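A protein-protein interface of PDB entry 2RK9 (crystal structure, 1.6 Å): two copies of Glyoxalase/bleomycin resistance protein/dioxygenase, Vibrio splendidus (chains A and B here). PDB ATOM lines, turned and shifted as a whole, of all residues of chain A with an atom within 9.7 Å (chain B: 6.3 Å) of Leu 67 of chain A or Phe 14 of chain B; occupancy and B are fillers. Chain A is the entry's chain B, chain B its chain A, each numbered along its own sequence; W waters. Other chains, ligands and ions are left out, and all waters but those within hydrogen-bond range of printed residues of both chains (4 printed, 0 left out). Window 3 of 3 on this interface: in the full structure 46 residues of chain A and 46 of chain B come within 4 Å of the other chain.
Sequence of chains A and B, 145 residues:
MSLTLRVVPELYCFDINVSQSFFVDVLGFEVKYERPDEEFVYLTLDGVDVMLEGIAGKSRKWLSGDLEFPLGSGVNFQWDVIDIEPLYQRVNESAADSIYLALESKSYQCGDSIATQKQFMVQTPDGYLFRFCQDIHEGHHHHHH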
ATOM      1  N   LEU A  67      19.032 -23.372  -1.011  1.00  0.00           N
ATOM      2  CA  LEU A  67      19.145 -24.171  -2.236  1.00  0.00           C
ATOM      3  C   LEU A  67      20.542 -24.068  -2.853  1.00  0.00           C
ATOM      4  O   LEU A  67      20.914 -23.007  -3.332  1.00  0.00           O
ATOM      5  CB  LEU A  67      18.092 -23.738  -3.261  1.00  0.00           C
ATOM      6  CG  LEU A  67      16.628 -23.870  -2.837  1.00  0.00           C
ATOM      7  CD1 LEU A  67      15.701 -23.398  -3.946  1.00  0.00           C
ATOM      8  CD2 LEU A  67      16.308 -25.306  -2.448  1.00  0.00           C
ATOM      9  N   GLU A  68      21.260 -25.140  -2.767  1.00  0.00           N
ATOM     10  CA  GLU A  68      22.632 -25.196  -3.254  1.00  0.00           C
ATOM     11  C   GLU A  68      22.955 -26.570  -3.832  1.00  0.00           C
ATOM     12  O   GLU A  68      22.562 -27.574  -3.237  1.00  0.00           O
ATOM     13  CB  GLU A  68      23.612 -24.842  -2.135  1.00  0.00           C
ATOM     14  CG  GLU A  68      23.418 -23.449  -1.560  1.00  0.00           C
ATOM     15  CD  GLU A  68      24.398 -23.136  -0.447  1.00  0.00           C
ATOM     16  OE1 GLU A  68      25.234 -24.008  -0.129  1.00  0.00           O
ATOM     17  OE2 GLU A  68      24.331 -22.020   0.110  1.00  0.00           O
ATOM     18  N   PHE A  69      23.604 -26.612  -4.977  1.00  0.00           N
ATOM     19  CA  PHE A  69      23.951 -27.887  -5.604  1.00  0.00           C
ATOM     20  C   PHE A  69      24.845 -28.682  -4.653  1.00  0.00           C
ATOM     21  O   PHE A  69      25.780 -28.136  -4.077  1.00  0.00           O
ATOM     22  CB  PHE A  69      24.697 -27.650  -6.918  1.00  0.00           C
ATOM     23  CG  PHE A  69      25.213 -28.912  -7.550  1.00  0.00           C
ATOM     24  CD1 PHE A  69      24.434 -29.622  -8.459  1.00  0.00           C
ATOM     25  CD2 PHE A  69      26.471 -29.405  -7.221  1.00  0.00           C
ATOM     26  CE1 PHE A  69      24.901 -30.803  -9.032  1.00  0.00           C
ATOM     27  CE2 PHE A  69      26.946 -30.587  -7.789  1.00  0.00           C
ATOM     28  CZ  PHE A  69      26.162 -31.285  -8.693  1.00  0.00           C
ATOM     29  N   PRO A  70      24.592 -29.989  -4.498  1.00  0.00           N
ATOM     30  CA  PRO A  70      23.524 -30.770  -5.136  1.00  0.00           C
ATOM     31  C   PRO A  70      22.239 -30.784  -4.311  1.00  0.00           C
ATOM     32  O   PRO A  70      22.280 -30.852  -3.092  1.00  0.00           O
ATOM     33  CB  PRO A  70      24.148 -32.153  -5.244  1.00  0.00           C
ATOM     34  CG  PRO A  70      24.920 -32.238  -3.957  1.00  0.00           C
ATOM     35  CD  PRO A  70      25.575 -30.878  -3.854  1.00  0.00           C
ATOM     36  N   LEU A  71      21.100 -30.715  -4.986  1.00  0.00           N
ATOM     37  CA  LEU A  71      19.816 -30.742  -4.299  1.00  0.00           C
ATOM     38  C   LEU A  71      19.368 -32.184  -4.098  1.00  0.00           C
ATOM     39  O   LEU A  71      19.945 -33.103  -4.681  1.00  0.00           O
ATOM     40  CB  LEU A  71      18.763 -29.998  -5.116  1.00  0.00           C
ATOM     41  CG  LEU A  71      19.017 -28.511  -5.331  1.00  0.00           C
ATOM     42  CD1 LEU A  71      17.983 -27.959  -6.309  1.00  0.00           C
ATOM     43  CD2 LEU A  71      18.954 -27.784  -3.984  1.00  0.00           C
ATOM     44  N   GLY A  72      18.348 -32.360  -3.257  1.00  0.00           N
ATOM     45  CA  GLY A  72      17.791 -33.678  -2.991  1.00  0.00           C
ATOM     46  C   GLY A  72      18.601 -34.637  -2.136  1.00  0.00           C
ATOM     47  O   GLY A  72      18.372 -35.846  -2.185  1.00  0.00           O
ATOM     48  N   SER A  73      19.534 -34.123  -1.343  1.00  0.00           N
ATOM     49  CA  SER A  73      20.350 -34.999  -0.513  1.00  0.00           C
ATOM     50  C   SER A  73      19.486 -35.947   0.307  1.00  0.00           C
ATOM     51  O   SER A  73      18.475 -35.547   0.882  1.00  0.00           O
ATOM     52  CB  SER A  73      21.250 -34.183   0.422  1.00  0.00           C
ATOM     53  OG  SER A  73      20.481 -33.397   1.315  1.00  0.00           O
ATOM     54  N   THR A 124      20.992 -35.832 -12.106  1.00  0.00           N
ATOM     55  CA  THR A 124      20.566 -34.766 -12.998  1.00  0.00           C
ATOM     56  C   THR A 124      21.453 -33.553 -12.717  1.00  0.00           C
ATOM     57  O   THR A 124      22.164 -33.516 -11.711  1.00  0.00           O
ATOM     58  CB  THR A 124      19.098 -34.398 -12.756  1.00  0.00           C
ATOM     59  OG1 THR A 124      18.977 -33.678 -11.524  1.00  0.00           O
ATOM     60  CG2 THR A 124      18.248 -35.665 -12.685  1.00  0.00           C
ATOM     61  N   PRO A 125      21.421 -32.541 -13.599  1.00  0.00           N
ATOM     62  CA  PRO A 125      22.250 -31.343 -13.402  1.00  0.00           C
ATOM     63  C   PRO A 125      22.108 -30.680 -12.032  1.00  0.00           C
ATOM     64  O   PRO A 125      23.071 -30.123 -11.498  1.00  0.00           O
ATOM     65  CB  PRO A 125      21.798 -30.422 -14.536  1.00  0.00           C
ATOM     66  CG  PRO A 125      21.389 -31.404 -15.628  1.00  0.00           C
ATOM     67  CD  PRO A 125      20.621 -32.438 -14.833  1.00  0.00           C
ATOM     68  N   ASP A 126      20.910 -30.742 -11.460  1.00  0.00           N
ATOM     69  CA  ASP A 126      20.654 -30.123 -10.162  1.00  0.00           C
ATOM     70  C   ASP A 126      21.141 -30.947  -8.975  1.00  0.00           C
ATOM     71  O   ASP A 126      21.178 -30.447  -7.852  1.00  0.00           O
ATOM     72  CB  ASP A 126      19.162 -29.848 -10.015  1.00  0.00           C
ATOM     73  CG  ASP A 126      18.626 -28.975 -11.130  1.00  0.00           C
ATOM     74  OD1 ASP A 126      18.932 -27.762 -11.153  1.00  0.00           O
ATOM     75  OD2 ASP A 126      17.908 -29.506 -12.001  1.00  0.00           O
ATOM     76  N   GLY A 127      21.507 -32.201  -9.226  1.00  0.00           N
ATOM     77  CA  GLY A 127      21.999 -33.056  -8.159  1.00  0.00           C
ATOM     78  C   GLY A 127      21.110 -34.224  -7.763  1.00  0.00           C
ATOM     79  O   GLY A 127      21.543 -35.083  -7.002  1.00  0.00           O
ATOM     80  N   TYR A 128      19.880 -34.265  -8.271  1.00  0.00           N
ATOM     81  CA  TYR A 128      18.945 -35.347  -7.937  1.00  0.00           C
ATOM     82  C   TYR A 128      19.398 -36.712  -8.448  1.00  0.00           C
ATOM     83  O   TYR A 128      19.884 -36.842  -9.569  1.00  0.00           O
ATOM     84  CB  TYR A 128      17.557 -35.042  -8.501  1.00  0.00           C
ATOM     85  CG  TYR A 128      16.971 -33.754  -7.987  1.00  0.00           C
ATOM     86  CD1 TYR A 128      16.602 -33.616  -6.646  1.00  0.00           C
ATOM     87  CD2 TYR A 128      16.784 -32.664  -8.838  1.00  0.00           C
ATOM     88  CE1 TYR A 128      16.068 -32.431  -6.172  1.00  0.00           C
ATOM     89  CE2 TYR A 128      16.246 -31.474  -8.366  1.00  0.00           C
ATOM     90  CZ  TYR A 128      15.892 -31.368  -7.036  1.00  0.00           C
ATOM     91  OH  TYR A 128      15.367 -30.195  -6.561  1.00  0.00           O
ATOM     92  N   TYR B  12      12.782 -28.637  -7.757  1.00  0.00           N
ATOM     93  CA  TYR B  12      13.157 -27.284  -8.058  1.00  0.00           C
ATOM     94  C   TYR B  12      14.474 -27.346  -8.825  1.00  0.00           C
ATOM     95  O   TYR B  12      15.360 -28.146  -8.510  1.00  0.00           O
ATOM     96  CB  TYR B  12      13.243 -26.478  -6.769  1.00  0.00           C
ATOM     97  CG  TYR B  12      11.867 -26.015  -6.338  1.00  0.00           C
ATOM     98  CD1 TYR B  12      11.061 -26.798  -5.518  1.00  0.00           C
ATOM     99  CD2 TYR B  12      11.347 -24.812  -6.803  1.00  0.00           C
ATOM    100  CE1 TYR B  12       9.767 -26.392  -5.174  1.00  0.00           C
ATOM    101  CE2 TYR B  12      10.070 -24.397  -6.469  1.00  0.00           C
ATOM    102  CZ  TYR B  12       9.280 -25.189  -5.655  1.00  0.00           C
ATOM    103  OH  TYR B  12       8.007 -24.779  -5.318  1.00  0.00           O
ATOM    104  N   CYS B  13      14.567 -26.531  -9.867  1.00  0.00           N
ATOM    105  CA  CYS B  13      15.741 -26.504 -10.727  1.00  0.00           C
ATOM    106  C   CYS B  13      16.373 -25.122 -10.786  1.00  0.00           C
ATOM    107  O   CYS B  13      15.678 -24.113 -10.844  1.00  0.00           O
ATOM    108  CB  CYS B  13      15.347 -26.945 -12.135  1.00  0.00           C
ATOM    109  SG  CYS B  13      14.550 -28.577 -12.188  1.00  0.00           S
ATOM    110  N   PHE B  14      17.701 -25.096 -10.794  1.00  0.00           N
ATOM    111  CA  PHE B  14      18.449 -23.848 -10.855  1.00  0.00           C
ATOM    112  C   PHE B  14      18.304 -23.175 -12.226  1.00  0.00           C
ATOM    113  O   PHE B  14      18.054 -21.971 -12.319  1.00  0.00           O
ATOM    114  CB  PHE B  14      19.927 -24.117 -10.570  1.00  0.00           C
ATOM    115  CG  PHE B  14      20.204 -24.571  -9.162  1.00  0.00           C
ATOM    116  CD1 PHE B  14      20.139 -23.671  -8.103  1.00  0.00           C
ATOM    117  CD2 PHE B  14      20.539 -25.897  -8.895  1.00  0.00           C
ATOM    118  CE1 PHE B  14      20.411 -24.083  -6.800  1.00  0.00           C
ATOM    119  CE2 PHE B  14      20.811 -26.319  -7.595  1.00  0.00           C
ATOM    120  CZ  PHE B  14      20.746 -25.410  -6.547  1.00  0.00           C
ATOM    121  N   ASP B  15      18.449 -23.972 -13.277  1.00  0.00           N
ATOM    122  CA  ASP B  15      18.359 -23.503 -14.657  1.00  0.00           C
ATOM    123  C   ASP B  15      17.325 -24.399 -15.347  1.00  0.00           C
ATOM    124  O   ASP B  15      17.658 -25.478 -15.834  1.00  0.00           O
ATOM    125  CB  ASP B  15      19.735 -23.657 -15.313  1.00  0.00           C
ATOM    126  CG  ASP B  15      19.857 -22.906 -16.625  1.00  0.00           C
ATOM    127  OD1 ASP B  15      18.991 -23.077 -17.503  1.00  0.00           O
ATOM    128  OD2 ASP B  15      20.845 -22.154 -16.772  1.00  0.00           O
ATOM    129  N   ILE B  16      16.074 -23.945 -15.381  1.00  0.00           N
ATOM    130  CA  ILE B  16      14.990 -24.737 -15.956  1.00  0.00           C
ATOM    131  C   ILE B  16      15.244 -25.290 -17.353  1.00  0.00           C
ATOM    132  O   ILE B  16      14.897 -26.437 -17.626  1.00  0.00           O
ATOM    133  CB  ILE B  16      13.640 -23.960 -15.938  1.00  0.00           C
ATOM    134  CG1 ILE B  16      12.477 -24.920 -16.242  1.00  0.00           C
ATOM    135  CG2 ILE B  16      13.658 -22.833 -16.959  1.00  0.00           C
ATOM    136  CD1 ILE B  16      12.311 -26.042 -15.217  1.00  0.00           C
ATOM    137  N   SER B  19      17.684 -28.199 -17.066  1.00  0.00           N
ATOM    138  CA  SER B  19      17.034 -29.361 -16.472  1.00  0.00           C
ATOM    139  C   SER B  19      16.024 -29.980 -17.431  1.00  0.00           C
ATOM    140  O   SER B  19      15.944 -31.201 -17.555  1.00  0.00           O
ATOM    141  CB  SER B  19      16.346 -28.956 -15.168  1.00  0.00           C
ATOM    142  OG  SER B  19      17.274 -28.362 -14.275  1.00  0.00           O
ATOM    143  N   GLU B  39       8.016 -21.007 -15.032  1.00  0.00           N
ATOM    144  CA  GLU B  39       9.136 -21.914 -15.290  1.00  0.00           C
ATOM    145  C   GLU B  39       8.756 -23.299 -14.775  1.00  0.00           C
ATOM    146  O   GLU B  39       9.580 -24.022 -14.216  1.00  0.00           O
ATOM    147  CB  GLU B  39      10.418 -21.434 -14.608  1.00  0.00           C
ATOM    148  CG  GLU B  39      10.957 -20.090 -15.108  1.00  0.00           C
ATOM    149  CD  GLU B  39      12.444 -19.935 -14.837  1.00  0.00           C
ATOM    150  OE1 GLU B  39      12.883 -20.375 -13.750  1.00  0.00           O
ATOM    151  OE2 GLU B  39      13.172 -19.364 -15.689  1.00  0.00           O
ATOM    152  N   GLU B  53      10.305 -27.211 -11.522  1.00  0.00           N
ATOM    153  CA  GLU B  53       9.949 -25.818 -11.252  1.00  0.00           C
ATOM    154  C   GLU B  53      11.237 -25.016 -11.095  1.00  0.00           C
ATOM    155  O   GLU B  53      12.015 -25.259 -10.177  1.00  0.00           O
ATOM    156  CB  GLU B  53       9.113 -25.730  -9.972  1.00  0.00           C
ATOM    157  CG  GLU B  53       8.864 -24.321  -9.441  1.00  0.00           C
ATOM    158  CD  GLU B  53       7.861 -23.542 -10.266  1.00  0.00           C
ATOM    159  OE1 GLU B  53       6.825 -24.123 -10.649  1.00  0.00           O
ATOM    160  OE2 GLU B  53       8.097 -22.341 -10.520  1.00  0.00           O
ATOM    161  N   GLY B  54      11.458 -24.070 -12.001  1.00  0.00           N
ATOM    162  CA  GLY B  54      12.660 -23.255 -11.950  1.00  0.00           C
ATOM    163  C   GLY B  54      12.654 -22.260 -10.807  1.00  0.00           C
ATOM    164  O   GLY B  54      11.598 -21.869 -10.318  1.00  0.00           O
ATOM    165  N   ILE B  55      13.838 -21.847 -10.376  1.00  0.00           N
ATOM    166  CA  ILE B  55      13.934 -20.885  -9.290  1.00  0.00           C
ATOM    167  C   ILE B  55      14.294 -19.519  -9.860  1.00  0.00           C
ATOM    168  O   ILE B  55      14.588 -19.398 -11.059  1.00  0.00           O
ATOM    169  CB  ILE B  55      15.011 -21.294  -8.276  1.00  0.00           C
ATOM    170  CG1 ILE B  55      14.844 -22.767  -7.890  1.00  0.00           C
ATOM    171  CG2 ILE B  55      14.882 -20.428  -7.029  1.00  0.00           C
ATOM    172  CD1 ILE B  55      16.156 -23.395  -7.468  1.00  0.00           C
ATOM    173  N   SER B  73      16.279 -31.213   0.132  1.00  0.00           N
ATOM    174  CA  SER B  73      16.127 -29.844  -0.352  1.00  0.00           C
ATOM    175  C   SER B  73      15.766 -29.795  -1.841  1.00  0.00           C
ATOM    176  O   SER B  73      16.334 -30.524  -2.659  1.00  0.00           O
ATOM    177  CB  SER B  73      17.408 -29.041  -0.098  1.00  0.00           C
ATOM    178  OG  SER B  73      18.497 -29.562  -0.840  1.00  0.00           O
ATOM    179  N   GLY B  74      14.802 -28.942  -2.177  1.00  0.00           N
ATOM    180  CA  GLY B  74      14.375 -28.794  -3.559  1.00  0.00           C
ATOM    181  C   GLY B  74      13.286 -29.755  -3.991  1.00  0.00           C
ATOM    182  O   GLY B  74      12.708 -29.595  -5.061  1.00  0.00           O
HETATM  183  O   HOH W   1      20.573 -27.330  -0.955  1.00  0.00           O
HETATM  184  O   HOH W   2      18.810 -31.488   1.486  1.00  0.00           O
HETATM  185  O   HOH W   3      19.370 -26.539 -13.467  1.00  0.00           O
HETATM  186  O   HOH W   4      20.442 -31.338  -1.023  1.00  0.00           O
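Among the printed residues, pairs that only touch across the chains: Leu 67 of chain A with Phe 14 of chain B, Leu 67 of chain A with Ile 55 of chain B, Leu 67 of chain A with Gly 74 of chain B, Glu 68 of chain A with Phe 14 of chain B, Phe 69 of chain A with Phe 14 of chain B, Leu 71 of chain A with Tyr 12 of chain B, Leu 71 of chain A with Phe 14 of chain B and Leu 71 of chain A with Ser 73 of chain B.
The side-chain hydroxyl (OG) of Ser 19 of chain B lies close to the side-chain sulfur (SG) of Cys 13 of chain B (3.4 Å).
The backbone NH of Cys 13 of chain B lies within hydrogen-bond range of the backbone carbonyl oxygen of Glu 53 of chain B.
The backbone carbonyl oxygen of Cys 13 of chain B lies within hydrogen-bond range of the backbone NH of Ile 55 of chain B.
The backbone carbonyl oxygen of Asp 15 of chain B is in hydrogen-bond range of the side-chain hydroxyl of Ser 19 of chain B.
N of Leu 71 of chain A lies within hydrogen-bond range of O of Asp 126 of chain A.
N of Tyr 128 of chain A lies within hydrogen-bond range of OG1 of Thr 124 of chain A, 3.4 Å away.
Position printed for both chains: 73.
Of the 14 pairs that touch across the chains among the printed residues, none has its exchanged pair printed and touching as well.
Hydrophobic or aromatic side chains of chain A that line the printed part of chain B: Leu 67, Leu 71 and Tyr 128.
Among the printed residues, no Asp or Glu carboxylate lies within 4 Å of a Lys or Arg side-chain nitrogen of the other chain.
Water W2 lies within hydrogen-bond range of OG of Ser 73 of chain A (2.5 Å) and N of Ser 73 of chain B (2.9 Å).
Water W4 lies within hydrogen-bond range of OG of Ser 73 of chain B (2.6 Å), O of Pro 70 of chain A (2.8 Å), N of Ser 73 of chain A (2.9 Å) and N of Gly 72 of chain A (3.2 Å).
Water W3 lies within hydrogen-bond range of OD1 of Asp 126 of chain A (2.7 Å), N of Asp 15 of chain B (2.7 Å), OG of Ser 19 of chain B (2.9 Å) and N of Phe 14 of chain B (3.5 Å).
Water W1 lies within hydrogen-bond range of N of Glu 68 of chain A (2.9 Å) and OG of Ser 73 of chain B (3.1 Å).
Of the printed residues of chain B, Glu 68 of chain A touches Phe 14 (3.7 Å).
Of the printed residues of chain B, Gly 72 of chain A touches Ser 73.
Pro 125 of chain A touches none of the printed residues of chain B.
Of the printed residues of chain A, Tyr 12 of chain B touches Leu 71 and Tyr 128.
Of chain A, only Leu 67 (3.7 Å), Glu 68 (3.7 Å), Phe 69 (3.5 Å), Leu 71 (3.5 Å) and Asp 126 (3.0 Å) come within 4 Å of Phe 14 of chain B.
No residue of chain A comes within 4 Å of Asp 15 of chain B.
Of chain A, only Leu 67 (3.6 Å) comes within 4 Å of Ile 55 of chain B.
Of the printed residues of chain A, Ser 73 of chain B touches Leu 71 and Gly 72.
The nearest residue of chain A that does not touch Phe 14 of chain B is Pro 125 of chain A (5.6 Å).
The backbone carbonyl oxygen (O) of Tyr 12 of chain B is in hydrogen-bond range of the side-chain hydroxyl (OH) of Tyr 128 of chain A (2.8 Å).
The side-chain sulfur (SG) of Cys 13 of chain B lies within hydrogen-bond range of the side-chain carboxylate (OD2) of Asp 126 of chain A (3.5 Å).
The side-chain carboxylate (OD1) of Asp 126 of chain A lies within hydrogen-bond range of the backbone NH (N) of Phe 14 of chain B (3.0 Å).
OG of Ser 19 of chain B sits at hydrogen-bond distance from OD2 of Asp 126 of chain A (2.6 Å).
The backbone NH (N) of Gly 72 of chain A is in hydrogen-bond range of the backbone carbonyl oxygen (O) of Ser 73 of chain B.
O of Gly 74 of chain B lies within hydrogen-bond range of OH of Tyr 128 of chain A (3.1 Å).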
